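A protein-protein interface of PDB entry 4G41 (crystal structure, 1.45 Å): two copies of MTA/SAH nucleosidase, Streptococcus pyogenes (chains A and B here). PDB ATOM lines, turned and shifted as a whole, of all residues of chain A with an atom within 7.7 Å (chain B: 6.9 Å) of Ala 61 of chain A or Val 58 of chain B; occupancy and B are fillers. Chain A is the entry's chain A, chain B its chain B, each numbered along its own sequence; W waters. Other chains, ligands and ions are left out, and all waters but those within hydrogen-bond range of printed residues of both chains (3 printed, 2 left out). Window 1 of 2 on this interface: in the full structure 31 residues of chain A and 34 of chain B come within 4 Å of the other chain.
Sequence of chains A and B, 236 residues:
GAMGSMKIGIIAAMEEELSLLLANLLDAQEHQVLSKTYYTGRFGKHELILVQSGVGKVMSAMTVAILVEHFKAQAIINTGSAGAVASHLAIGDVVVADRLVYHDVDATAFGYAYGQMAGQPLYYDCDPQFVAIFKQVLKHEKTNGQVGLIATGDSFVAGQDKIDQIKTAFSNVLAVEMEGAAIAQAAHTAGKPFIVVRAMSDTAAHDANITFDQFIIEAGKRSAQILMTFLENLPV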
ATOM      1  N   ILE A  11      33.849 -33.351   6.306  1.00  0.00           N
ATOM      2  CA  ILE A  11      32.401 -33.674   6.556  1.00  0.00           C
ATOM      3  C   ILE A  11      32.130 -34.862   5.675  1.00  0.00           C
ATOM      4  O   ILE A  11      31.959 -34.673   4.469  1.00  0.00           O
ATOM      5  CB  ILE A  11      31.522 -32.464   6.243  1.00  0.00           C
ATOM      6  CG1 ILE A  11      32.018 -31.213   7.067  1.00  0.00           C
ATOM      7  CG2 ILE A  11      30.066 -32.870   6.491  1.00  0.00           C
ATOM      8  CD1 ILE A  11      31.252 -29.970   6.612  1.00  0.00           C
ATOM      9  N   GLY A  56      20.839 -32.191   4.868  1.00  0.00           N
ATOM     10  CA  GLY A  56      20.154 -30.956   4.587  1.00  0.00           C
ATOM     11  C   GLY A  56      20.931 -29.698   4.826  1.00  0.00           C
ATOM     12  O   GLY A  56      22.015 -29.716   5.391  1.00  0.00           O
ATOM     13  N   LYS A  57      20.302 -28.569   4.559  1.00  0.00           N
ATOM     14  CA  LYS A  57      21.021 -27.277   4.565  1.00  0.00           C
ATOM     15  C   LYS A  57      21.400 -26.815   5.987  1.00  0.00           C
ATOM     16  O   LYS A  57      22.531 -26.394   6.192  1.00  0.00           O
ATOM     17  CB  LYS A  57      20.165 -26.187   3.890  1.00  0.00           C
ATOM     18  CG  LYS A  57      19.927 -26.431   2.394  1.00  0.00           C
ATOM     19  CD  LYS A  57      19.160 -25.247   1.830  1.00  0.00           C
ATOM     20  CE  LYS A  57      18.702 -25.602   0.435  1.00  0.00           C
ATOM     21  NZ  LYS A  57      18.084 -24.386  -0.305  1.00  0.00           N
ATOM     22  N   VAL A  58      20.438 -26.894   6.908  1.00  0.00           N
ATOM     23  CA  VAL A  58      20.674 -26.352   8.262  1.00  0.00           C
ATOM     24  C   VAL A  58      21.775 -27.205   8.929  1.00  0.00           C
ATOM     25  O   VAL A  58      22.687 -26.595   9.505  1.00  0.00           O
ATOM     26  CB  VAL A  58      19.362 -26.299   9.075  1.00  0.00           C
ATOM     27  CG1 VAL A  58      19.644 -26.122  10.554  1.00  0.00           C
ATOM     28  CG2 VAL A  58      18.509 -25.133   8.536  1.00  0.00           C
ATOM     29  N   MET A  59      21.749 -28.508   8.913  1.00  0.00           N
ATOM     30  CA  MET A  59      22.785 -29.250   9.656  1.00  0.00           C
ATOM     31  C   MET A  59      24.132 -29.035   8.987  1.00  0.00           C
ATOM     32  O   MET A  59      25.156 -28.896   9.686  1.00  0.00           O
ATOM     33  CB  MET A  59      22.422 -30.733   9.685  1.00  0.00           C
ATOM     34  CG  MET A  59      21.130 -30.993  10.458  1.00  0.00           C
ATOM     35  SD  MET A  59      20.842 -29.981  11.956  1.00  0.00           S
ATOM     36  CE  MET A  59      22.099 -30.430  13.173  1.00  0.00           C
ATOM     37  N   SER A  60      24.185 -28.886   7.662  1.00  0.00           N
ATOM     38  CA  SER A  60      25.453 -28.580   6.946  1.00  0.00           C
ATOM     39  C   SER A  60      25.991 -27.242   7.402  1.00  0.00           C
ATOM     40  O   SER A  60      27.208 -27.091   7.675  1.00  0.00           O
ATOM     41  CB  SER A  60      25.137 -28.530   5.451  1.00  0.00           C
ATOM     42  OG  SER A  60      24.772 -29.845   4.994  1.00  0.00           O
ATOM     43  N   ALA A  61      25.092 -26.244   7.504  1.00  0.00           N
ATOM     44  CA  ALA A  61      25.572 -24.847   7.835  1.00  0.00           C
ATOM     45  C   ALA A  61      26.087 -24.855   9.290  1.00  0.00           C
ATOM     46  O   ALA A  61      27.148 -24.205   9.580  1.00  0.00           O
ATOM     47  CB  ALA A  61      24.371 -23.923   7.725  1.00  0.00           C
ATOM     48  N   MET A  62      25.409 -25.575  10.203  1.00  0.00           N
ATOM     49  CA  MET A  62      25.919 -25.645  11.610  1.00  0.00           C
ATOM     50  C   MET A  62      27.269 -26.320  11.644  1.00  0.00           C
ATOM     51  O   MET A  62      28.139 -25.902  12.410  1.00  0.00           O
ATOM     52  CB  MET A  62      24.933 -26.388  12.498  1.00  0.00           C
ATOM     53  CG  MET A  62      23.541 -25.705  12.600  1.00  0.00           C
ATOM     54  SD  MET A  62      22.451 -26.554  13.722  1.00  0.00           S
ATOM     55  CE  MET A  62      23.119 -26.033  15.266  1.00  0.00           C
ATOM     56  N   THR A  63      27.450 -27.407  10.912  1.00  0.00           N
ATOM     57  CA  THR A  63      28.725 -28.124  10.919  1.00  0.00           C
ATOM     58  C   THR A  63      29.829 -27.240  10.422  1.00  0.00           C
ATOM     59  O   THR A  63      30.910 -27.182  11.058  1.00  0.00           O
ATOM     60  CB  THR A  63      28.648 -29.348   9.997  1.00  0.00           C
ATOM     61  OG1 THR A  63      27.652 -30.220  10.476  1.00  0.00           O
ATOM     62  CG2 THR A  63      29.963 -30.135  10.053  1.00  0.00           C
ATOM     63  N   VAL A  64      29.649 -26.469   9.358  1.00  0.00           N
ATOM     64  CA  VAL A  64      30.742 -25.641   8.900  1.00  0.00           C
ATOM     65  C   VAL A  64      30.984 -24.550   9.935  1.00  0.00           C
ATOM     66  O   VAL A  64      32.170 -24.247  10.245  1.00  0.00           O
ATOM     67  CB  VAL A  64      30.394 -24.981   7.542  1.00  0.00           C
ATOM     68  CG1 VAL A  64      31.427 -23.885   7.228  1.00  0.00           C
ATOM     69  CG2 VAL A  64      30.380 -26.055   6.427  1.00  0.00           C
ATOM     70  N   ALA A  65      29.934 -23.960  10.486  1.00  0.00           N
ATOM     71  CA  ALA A  65      30.174 -22.893  11.489  1.00  0.00           C
ATOM     72  C   ALA A  65      30.981 -23.405  12.681  1.00  0.00           C
ATOM     73  O   ALA A  65      31.877 -22.684  13.205  1.00  0.00           O
ATOM     74  CB  ALA A  65      28.804 -22.283  11.941  1.00  0.00           C
ATOM     75  N   ILE A  66      30.647 -24.606  13.141  1.00  0.00           N
ATOM     76  CA  ILE A  66      31.370 -25.184  14.298  1.00  0.00           C
ATOM     77  C   ILE A  66      32.786 -25.601  13.911  1.00  0.00           C
ATOM     78  O   ILE A  66      33.746 -25.322  14.710  1.00  0.00           O
ATOM     79  CB  ILE A  66      30.589 -26.351  14.934  1.00  0.00           C
ATOM     80  CG1 ILE A  66      29.303 -25.781  15.581  1.00  0.00           C
ATOM     81  CG2 ILE A  66      31.432 -27.182  15.921  1.00  0.00           C
ATOM     82  CD1 ILE A  66      29.606 -24.739  16.709  1.00  0.00           C
ATOM     83  N   LEU A  67      33.004 -26.173  12.718  1.00  0.00           N
ATOM     84  CA  LEU A  67      34.359 -26.547  12.328  1.00  0.00           C
ATOM     85  C   LEU A  67      35.211 -25.331  12.310  1.00  0.00           C
ATOM     86  O   LEU A  67      36.384 -25.385  12.766  1.00  0.00           O
ATOM     87  CB  LEU A  67      34.331 -27.228  10.954  1.00  0.00           C
ATOM     88  CG  LEU A  67      33.824 -28.661  10.940  1.00  0.00           C
ATOM     89  CD1 LEU A  67      33.666 -29.153   9.489  1.00  0.00           C
ATOM     90  CD2 LEU A  67      34.761 -29.553  11.762  1.00  0.00           C
ATOM     91  N   TYR A 102      22.058 -24.085  -5.896  1.00  0.00           N
ATOM     92  CA  TYR A 102      20.774 -24.626  -5.352  1.00  0.00           C
ATOM     93  C   TYR A 102      19.805 -24.807  -6.472  1.00  0.00           C
ATOM     94  O   TYR A 102      19.601 -23.908  -7.329  1.00  0.00           O
ATOM     95  CB  TYR A 102      20.176 -23.634  -4.353  1.00  0.00           C
ATOM     96  CG  TYR A 102      20.999 -23.528  -3.069  1.00  0.00           C
ATOM     97  CD1 TYR A 102      21.074 -24.632  -2.230  1.00  0.00           C
ATOM     98  CD2 TYR A 102      21.480 -22.284  -2.646  1.00  0.00           C
ATOM     99  CE1 TYR A 102      21.691 -24.541  -1.018  1.00  0.00           C
ATOM    100  CE2 TYR A 102      22.140 -22.176  -1.418  1.00  0.00           C
ATOM    101  CZ  TYR A 102      22.218 -23.327  -0.588  1.00  0.00           C
ATOM    102  OH  TYR A 102      22.890 -23.228   0.643  1.00  0.00           O
ATOM    103  N   MET A 117      20.286 -17.519  -4.142  1.00  0.00           N
ATOM    104  CA  MET A 117      19.863 -16.999  -2.843  1.00  0.00           C
ATOM    105  C   MET A 117      20.052 -15.494  -2.736  1.00  0.00           C
ATOM    106  O   MET A 117      21.043 -15.002  -3.260  1.00  0.00           O
ATOM    107  CB  MET A 117      20.625 -17.784  -1.720  1.00  0.00           C
ATOM    108  CG  MET A 117      20.284 -17.361  -0.316  1.00  0.00           C
ATOM    109  SD  MET A 117      18.518 -17.246   0.178  1.00  0.00           S
ATOM    110  CE  MET A 117      18.011 -18.945  -0.089  1.00  0.00           C
ATOM    111  N   GLN A 120      23.595 -13.657  -2.410  1.00  0.00           N
ATOM    112  CA  GLN A 120      24.650 -14.631  -2.778  1.00  0.00           C
ATOM    113  C   GLN A 120      24.824 -14.692  -4.259  1.00  0.00           C
ATOM    114  O   GLN A 120      23.900 -14.306  -4.969  1.00  0.00           O
ATOM    115  CB  GLN A 120      24.192 -16.036  -2.299  1.00  0.00           C
ATOM    116  CG  GLN A 120      23.910 -16.151  -0.800  1.00  0.00           C
ATOM    117  CD  GLN A 120      25.097 -15.926   0.080  1.00  0.00           C
ATOM    118  OE1 GLN A 120      24.913 -15.581   1.298  1.00  0.00           O
ATOM    119  NE2 GLN A 120      26.267 -16.237  -0.398  1.00  0.00           N
ATOM    120  N   TYR A 124      28.490 -21.212  -6.376  1.00  0.00           N
ATOM    121  CA  TYR A 124      29.574 -21.112  -5.447  1.00  0.00           C
ATOM    122  C   TYR A 124      30.800 -21.857  -6.000  1.00  0.00           C
ATOM    123  O   TYR A 124      30.632 -22.919  -6.638  1.00  0.00           O
ATOM    124  CB  TYR A 124      29.197 -21.776  -4.105  1.00  0.00           C
ATOM    125  CG  TYR A 124      27.958 -21.158  -3.516  1.00  0.00           C
ATOM    126  CD1 TYR A 124      28.020 -19.975  -2.686  1.00  0.00           C
ATOM    127  CD2 TYR A 124      26.656 -21.694  -3.822  1.00  0.00           C
ATOM    128  CE1 TYR A 124      26.862 -19.375  -2.192  1.00  0.00           C
ATOM    129  CE2 TYR A 124      25.472 -21.041  -3.320  1.00  0.00           C
ATOM    130  CZ  TYR A 124      25.593 -19.911  -2.499  1.00  0.00           C
ATOM    131  OH  TYR A 124      24.463 -19.296  -1.976  1.00  0.00           O
ATOM    132  N   ASP A 154      16.924 -29.050  -0.367  1.00  0.00           N
ATOM    133  CA  ASP A 154      16.481 -29.662   0.906  1.00  0.00           C
ATOM    134  C   ASP A 154      15.352 -30.677   0.666  1.00  0.00           C
ATOM    135  O   ASP A 154      14.421 -30.830   1.447  1.00  0.00           O
ATOM    136  CB  ASP A 154      15.992 -28.564   1.868  1.00  0.00           C
ATOM    137  CG  ASP A 154      16.887 -28.380   3.110  1.00  0.00           C
ATOM    138  OD1 ASP A 154      17.910 -29.036   3.153  1.00  0.00           O
ATOM    139  OD2 ASP A 154      16.391 -27.585   3.964  1.00  0.00           O
ATOM    140  N   GLU A 179      23.345 -31.590   0.405  1.00  0.00           N
ATOM    141  CA  GLU A 179      24.196 -30.743   1.335  1.00  0.00           C
ATOM    142  C   GLU A 179      25.230 -29.882   0.595  1.00  0.00           C
ATOM    143  O   GLU A 179      25.659 -28.828   1.182  1.00  0.00           O
ATOM    144  CB  GLU A 179      25.060 -31.686   2.219  1.00  0.00           C
ATOM    145  CG  GLU A 179      24.241 -32.435   3.299  1.00  0.00           C
ATOM    146  CD  GLU A 179      23.538 -33.668   2.730  1.00  0.00           C
ATOM    147  OE1 GLU A 179      24.233 -34.451   2.016  1.00  0.00           O
ATOM    148  OE2 GLU A 179      22.379 -33.937   3.096  1.00  0.00           O
ATOM    149  N   ALA A 181      25.772 -27.511  -1.843  1.00  0.00           N
ATOM    150  CA  ALA A 181      25.760 -26.043  -1.988  1.00  0.00           C
ATOM    151  C   ALA A 181      25.603 -25.345  -0.619  1.00  0.00           C
ATOM    152  O   ALA A 181      25.970 -24.154  -0.497  1.00  0.00           O
ATOM    153  CB  ALA A 181      24.635 -25.531  -2.924  1.00  0.00           C
ATOM    154  N   ALA A 182      24.972 -26.042   0.377  1.00  0.00           N
ATOM    155  CA  ALA A 182      24.924 -25.398   1.728  1.00  0.00           C
ATOM    156  C   ALA A 182      26.294 -25.382   2.367  1.00  0.00           C
ATOM    157  O   ALA A 182      26.649 -24.400   2.997  1.00  0.00           O
ATOM    158  CB  ALA A 182      23.895 -26.206   2.608  1.00  0.00           C
ATOM    159  N   ILE A 183      27.066 -26.471   2.222  1.00  0.00           N
ATOM    160  CA  ILE A 183      28.478 -26.496   2.658  1.00  0.00           C
ATOM    161  C   ILE A 183      29.222 -25.336   1.976  1.00  0.00           C
ATOM    162  O   ILE A 183      29.980 -24.599   2.628  1.00  0.00           O
ATOM    163  CB  ILE A 183      29.153 -27.847   2.292  1.00  0.00           C
ATOM    164  CG1 ILE A 183      28.494 -29.028   3.025  1.00  0.00           C
ATOM    165  CG2 ILE A 183      30.718 -27.787   2.417  1.00  0.00           C
ATOM    166  CD1 ILE A 183      28.721 -29.135   4.499  1.00  0.00           C
ATOM    167  N   ALA A 184      29.025 -25.218   0.673  1.00  0.00           N
ATOM    168  CA  ALA A 184      29.722 -24.172  -0.105  1.00  0.00           C
ATOM    169  C   ALA A 184      29.306 -22.802   0.365  1.00  0.00           C
ATOM    170  O   ALA A 184      30.189 -21.943   0.579  1.00  0.00           O
ATOM    171  CB  ALA A 184      29.314 -24.381  -1.536  1.00  0.00           C
ATOM    172  N   GLN A 185      27.991 -22.558   0.521  1.00  0.00           N
ATOM    173  CA  GLN A 185      27.584 -21.234   0.906  1.00  0.00           C
ATOM    174  C   GLN A 185      28.124 -20.894   2.306  1.00  0.00           C
ATOM    175  O   GLN A 185      28.611 -19.764   2.532  1.00  0.00           O
ATOM    176  CB  GLN A 185      26.033 -21.197   0.887  1.00  0.00           C
ATOM    177  CG  GLN A 185      25.539 -19.802   1.300  1.00  0.00           C
ATOM    178  CD  GLN A 185      24.034 -19.742   1.530  1.00  0.00           C
ATOM    179  OE1 GLN A 185      23.280 -20.733   1.339  1.00  0.00           O
ATOM    180  NE2 GLN A 185      23.554 -18.534   1.955  1.00  0.00           N
ATOM    181  N   ALA A 186      28.125 -21.862   3.249  1.00  0.00           N
ATOM    182  CA  ALA A 186      28.609 -21.593   4.576  1.00  0.00           C
ATOM    183  C   ALA A 186      30.159 -21.386   4.576  1.00  0.00           C
ATOM    184  O   ALA A 186      30.665 -20.479   5.267  1.00  0.00           O
ATOM    185  CB  ALA A 186      28.203 -22.757   5.480  1.00  0.00           C
ATOM    186  N   ALA A 187      30.878 -22.267   3.879  1.00  0.00           N
ATOM    187  CA  ALA A 187      32.330 -22.124   3.922  1.00  0.00           C
ATOM    188  C   ALA A 187      32.730 -20.839   3.223  1.00  0.00           C
ATOM    189  O   ALA A 187      33.670 -20.148   3.677  1.00  0.00           O
ATOM    190  CB  ALA A 187      32.990 -23.325   3.220  1.00  0.00           C
ATOM    191  N   THR A 189      31.012 -18.017   3.072  1.00  0.00           N
ATOM    192  CA  THR A 189      30.676 -16.906   4.034  1.00  0.00           C
ATOM    193  C   THR A 189      31.768 -16.791   5.047  1.00  0.00           C
ATOM    194  O   THR A 189      32.208 -15.689   5.451  1.00  0.00           O
ATOM    195  CB  THR A 189      29.348 -17.335   4.782  1.00  0.00           C
ATOM    196  OG1 THR A 189      28.352 -17.270   3.823  1.00  0.00           O
ATOM    197  CG2 THR A 189      29.017 -16.360   5.942  1.00  0.00           C
ATOM    198  N   LEU B  34      33.215 -15.156  12.186  1.00  0.00           N
ATOM    199  CA  LEU B  34      32.913 -15.767  10.855  1.00  0.00           C
ATOM    200  C   LEU B  34      32.335 -14.726   9.894  1.00  0.00           C
ATOM    201  O   LEU B  34      31.351 -14.993   9.146  1.00  0.00           O
ATOM    202  CB  LEU B  34      31.902 -16.982  10.970  1.00  0.00           C
ATOM    203  CG  LEU B  34      32.415 -18.213  11.622  1.00  0.00           C
ATOM    204  CD1 LEU B  34      31.377 -19.291  11.316  1.00  0.00           C
ATOM    205  CD2 LEU B  34      33.748 -18.519  11.026  1.00  0.00           C
ATOM    206  N   SER B  53      21.844 -11.852  10.198  1.00  0.00           N
ATOM    207  CA  SER B  53      22.423 -13.114   9.689  1.00  0.00           C
ATOM    208  C   SER B  53      22.642 -13.125   8.202  1.00  0.00           C
ATOM    209  O   SER B  53      23.555 -13.811   7.702  1.00  0.00           O
ATOM    210  CB  SER B  53      21.534 -14.298  10.065  1.00  0.00           C
ATOM    211  OG  SER B  53      20.202 -14.113   9.507  1.00  0.00           O
ATOM    212  N   GLY B  54      21.795 -12.394   7.492  1.00  0.00           N
ATOM    213  CA  GLY B  54      21.653 -12.669   6.058  1.00  0.00           C
ATOM    214  C   GLY B  54      20.453 -13.584   5.852  1.00  0.00           C
ATOM    215  O   GLY B  54      19.991 -14.211   6.774  1.00  0.00           O
ATOM    216  N   VAL B  55      19.926 -13.571   4.588  1.00  0.00           N
ATOM    217  CA  VAL B  55      18.666 -14.289   4.326  1.00  0.00           C
ATOM    218  C   VAL B  55      18.853 -15.770   4.130  1.00  0.00           C
ATOM    219  O   VAL B  55      19.895 -16.213   3.560  1.00  0.00           O
ATOM    220  CB  VAL B  55      18.086 -13.702   3.002  1.00  0.00           C
ATOM    221  CG1 VAL B  55      16.936 -14.549   2.443  1.00  0.00           C
ATOM    222  CG2 VAL B  55      17.638 -12.264   3.183  1.00  0.00           C
ATOM    223  N   GLY B  56      17.866 -16.508   4.621  1.00  0.00           N
ATOM    224  CA  GLY B  56      17.727 -17.919   4.256  1.00  0.00           C
ATOM    225  C   GLY B  56      18.190 -18.942   5.287  1.00  0.00           C
ATOM    226  O   GLY B  56      18.714 -18.546   6.375  1.00  0.00           O
ATOM    227  N   LYS B  57      18.080 -20.210   4.920  1.00  0.00           N
ATOM    228  CA  LYS B  57      18.300 -21.272   5.919  1.00  0.00           C
ATOM    229  C   LYS B  57      19.753 -21.374   6.365  1.00  0.00           C
ATOM    230  O   LYS B  57      19.969 -21.461   7.565  1.00  0.00           O
ATOM    231  CB  LYS B  57      17.910 -22.659   5.291  1.00  0.00           C
ATOM    232  CG  LYS B  57      16.425 -22.796   5.003  1.00  0.00           C
ATOM    233  CD  LYS B  57      16.170 -24.189   4.447  1.00  0.00           C
ATOM    234  CE  LYS B  57      14.687 -24.317   4.060  1.00  0.00           C
ATOM    235  NZ  LYS B  57      14.468 -25.750   3.545  1.00  0.00           N
ATOM    236  N   VAL B  58      20.691 -21.317   5.406  1.00  0.00           N
ATOM    237  CA  VAL B  58      22.112 -21.545   5.781  1.00  0.00           C
ATOM    238  C   VAL B  58      22.524 -20.323   6.605  1.00  0.00           C
ATOM    239  O   VAL B  58      23.181 -20.551   7.664  1.00  0.00           O
ATOM    240  CB  VAL B  58      22.932 -21.715   4.518  1.00  0.00           C
ATOM    241  CG1 VAL B  58      24.425 -21.508   4.786  1.00  0.00           C
ATOM    242  CG2 VAL B  58      22.640 -23.104   3.918  1.00  0.00           C
ATOM    243  N   MET B  59      22.278 -19.089   6.150  1.00  0.00           N
ATOM    244  CA  MET B  59      22.848 -17.986   6.875  1.00  0.00           C
ATOM    245  C   MET B  59      22.341 -17.929   8.313  1.00  0.00           C
ATOM    246  O   MET B  59      23.112 -17.667   9.308  1.00  0.00           O
ATOM    247  CB  MET B  59      22.534 -16.648   6.249  1.00  0.00           C
ATOM    248  CG  MET B  59      23.172 -16.569   4.851  1.00  0.00           C
ATOM    249  SD  MET B  59      24.937 -16.849   4.682  1.00  0.00           S
ATOM    250  CE  MET B  59      25.585 -15.381   5.342  1.00  0.00           C
ATOM    251  N   SER B  60      21.038 -18.137   8.494  1.00  0.00           N
ATOM    252  CA  SER B  60      20.416 -18.030   9.807  1.00  0.00           C
ATOM    253  C   SER B  60      20.944 -19.170  10.691  1.00  0.00           C
ATOM    254  O   SER B  60      21.194 -18.971  11.907  1.00  0.00           O
ATOM    255  CB  SER B  60      18.916 -17.946   9.754  1.00  0.00           C
ATOM    256  OG  SER B  60      18.347 -19.084   9.142  1.00  0.00           O
ATOM    257  N   ALA B  61      21.039 -20.395  10.176  1.00  0.00           N
ATOM    258  CA  ALA B  61      21.511 -21.517  10.990  1.00  0.00           C
ATOM    259  C   ALA B  61      22.950 -21.340  11.411  1.00  0.00           C
ATOM    260  O   ALA B  61      23.272 -21.699  12.545  1.00  0.00           O
ATOM    261  CB  ALA B  61      21.382 -22.824  10.177  1.00  0.00           C
ATOM    262  N   MET B  62      23.785 -20.735  10.564  1.00  0.00           N
ATOM    263  CA  MET B  62      25.184 -20.481  11.052  1.00  0.00           C
ATOM    264  C   MET B  62      25.140 -19.623  12.299  1.00  0.00           C
ATOM    265  O   MET B  62      25.909 -19.872  13.283  1.00  0.00           O
ATOM    266  CB  MET B  62      25.948 -19.743  10.024  1.00  0.00           C
ATOM    267  CG  MET B  62      26.285 -20.636   8.787  1.00  0.00           C
ATOM    268  SD  MET B  62      27.354 -19.816   7.568  1.00  0.00           S
ATOM    269  CE  MET B  62      28.898 -20.006   8.342  1.00  0.00           C
ATOM    270  N   THR B  63      24.301 -18.586  12.289  1.00  0.00           N
ATOM    271  CA  THR B  63      24.294 -17.638  13.453  1.00  0.00           C
ATOM    272  C   THR B  63      23.745 -18.310  14.662  1.00  0.00           C
ATOM    273  O   THR B  63      24.175 -18.008  15.804  1.00  0.00           O
ATOM    274  CB  THR B  63      23.553 -16.294  13.179  1.00  0.00           C
ATOM    275  OG1 THR B  63      22.194 -16.545  12.869  1.00  0.00           O
ATOM    276  CG2 THR B  63      24.231 -15.521  12.066  1.00  0.00           C
ATOM    277  N   ALA B  65      24.335 -21.492  15.519  1.00  0.00           N
ATOM    278  CA  ALA B  65      25.513 -22.250  16.074  1.00  0.00           C
ATOM    279  C   ALA B  65      26.503 -21.306  16.758  1.00  0.00           C
ATOM    280  O   ALA B  65      26.999 -21.673  17.824  1.00  0.00           O
ATOM    281  CB  ALA B  65      26.187 -23.015  14.868  1.00  0.00           C
ATOM    282  N   ASP B 154      13.394 -21.822   1.505  1.00  0.00           N
ATOM    283  CA  ASP B 154      14.431 -20.988   0.892  1.00  0.00           C
ATOM    284  C   ASP B 154      13.894 -20.291  -0.381  1.00  0.00           C
ATOM    285  O   ASP B 154      14.584 -20.221  -1.415  1.00  0.00           O
ATOM    286  CB  ASP B 154      15.663 -21.818   0.604  1.00  0.00           C
ATOM    287  CG  ASP B 154      16.813 -21.588   1.593  1.00  0.00           C
ATOM    288  OD1 ASP B 154      16.701 -20.677   2.436  1.00  0.00           O
ATOM    289  OD2 ASP B 154      17.853 -22.262   1.387  1.00  0.00           O
ATOM    290  N   MET B 178      11.744 -17.097   5.408  1.00  0.00           N
ATOM    291  CA  MET B 178      12.923 -17.839   4.908  1.00  0.00           C
ATOM    292  C   MET B 178      13.906 -18.255   5.989  1.00  0.00           C
ATOM    293  O   MET B 178      14.928 -18.828   5.669  1.00  0.00           O
ATOM    294  CB  MET B 178      13.597 -17.099   3.768  1.00  0.00           C
ATOM    295  CG  MET B 178      12.629 -16.888   2.575  1.00  0.00           C
ATOM    296  SD  MET B 178      13.329 -15.750   1.322  1.00  0.00           S
ATOM    297  CE  MET B 178      14.666 -16.723   0.708  1.00  0.00           C
ATOM    298  N   ALA B 182      14.404 -22.773  10.120  1.00  0.00           N
ATOM    299  CA  ALA B 182      15.826 -23.062  10.122  1.00  0.00           C
ATOM    300  C   ALA B 182      16.427 -22.713  11.483  1.00  0.00           C
ATOM    301  O   ALA B 182      17.226 -23.496  12.027  1.00  0.00           O
ATOM    302  CB  ALA B 182      16.547 -22.225   9.014  1.00  0.00           C
HETATM  303  O   HOH W   1      21.991 -14.967   2.054  1.00  0.00           O
HETATM  304  O   HOH W   2      20.106 -21.193   2.408  1.00  0.00           O
HETATM  305  O   HOH W   3      15.225 -25.307   0.710  1.00  0.00           O
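The side-chain amino group (NZ) of Lys 57 of chain A lies within salt-bridge range of the side-chain carboxylate (OD2) of Asp 154 of chain B (2.7 Å). The side-chain amide oxygen of Gln 120 of chain A lies close to the side-chain sulfur of Met 59 of chain B (3.6 Å). The side-chain amino group (NZ) of Lys 57 of chain B is in salt-bridge range of the side-chain carboxylate (OD2) of Asp 154 of chain A (2.7 Å). The side-chain sulfur (SD) of Met 59 of chain B sits at hydrogen-bond distance from the side-chain amide nitrogen (NE2) of Gln 185 of chain A (3.5 Å). SD of Met 59 of chain B lies within hydrogen-bond range of OG1 of Thr 189 of chain A. The side-chain sulfur (SD) of Met 117 of chain A sits close to the backbone carbonyl oxygen (O) of Val 55 of chain B.
O of Lys 57 of chain B lies within hydrogen-bond range of OG of Ser 60 of chain B, at 3.3 Å. N of Lys 57 of chain B sits at hydrogen-bond distance from OD1 of Asp 154 of chain B (2.9 Å).
Printed residues of chain A within 4 Å of Met 59 of chain B: Gln 120 (3.6 Å), Gln 185 (3.5 Å) and Thr 189 (3.5 Å). Printed residues of chain A within 4 Å of Met 178 of chain B: Met 117 (3.9 Å). The nearest printed residue of chain B that does not touch Ala 61 of chain A is Ala 61 of chain B (4.02 Å). The nearest printed residue of chain B that does not touch Gln 185 of chain A is Val 55 of chain B (4.6 Å).
Of the 27 printed residues of chain A, 12 touch a printed residue of chain B. Hydrophobic or aromatic side chains of chain B within 4 Å of the printed part of chain A: Leu 34, Val 55, Val 58, Met 59, Ala 61, Met 62, Ala 65, Met 178 and Ala 182. Among the printed residues, 21 pairs touch across the chains.
Val 58 of chain A touches Ala 61 of chain B, and with the chains exchanged Ala 61 of chain A touches Val 58 of chain B. Positions printed for both chains: 56, 57, 58, 59, 60, 61, 62, 63, 65, 154 and 182.
Water W1 bridges the backbone carbonyl oxygen (O) of Val 55 of chain B and the side-chain amide oxygen (OE1) of Gln 120 of chain A. Water W3 lies within hydrogen-bond range of NZ of Lys 57 of chain B and NZ of Lys 57 of chain A.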
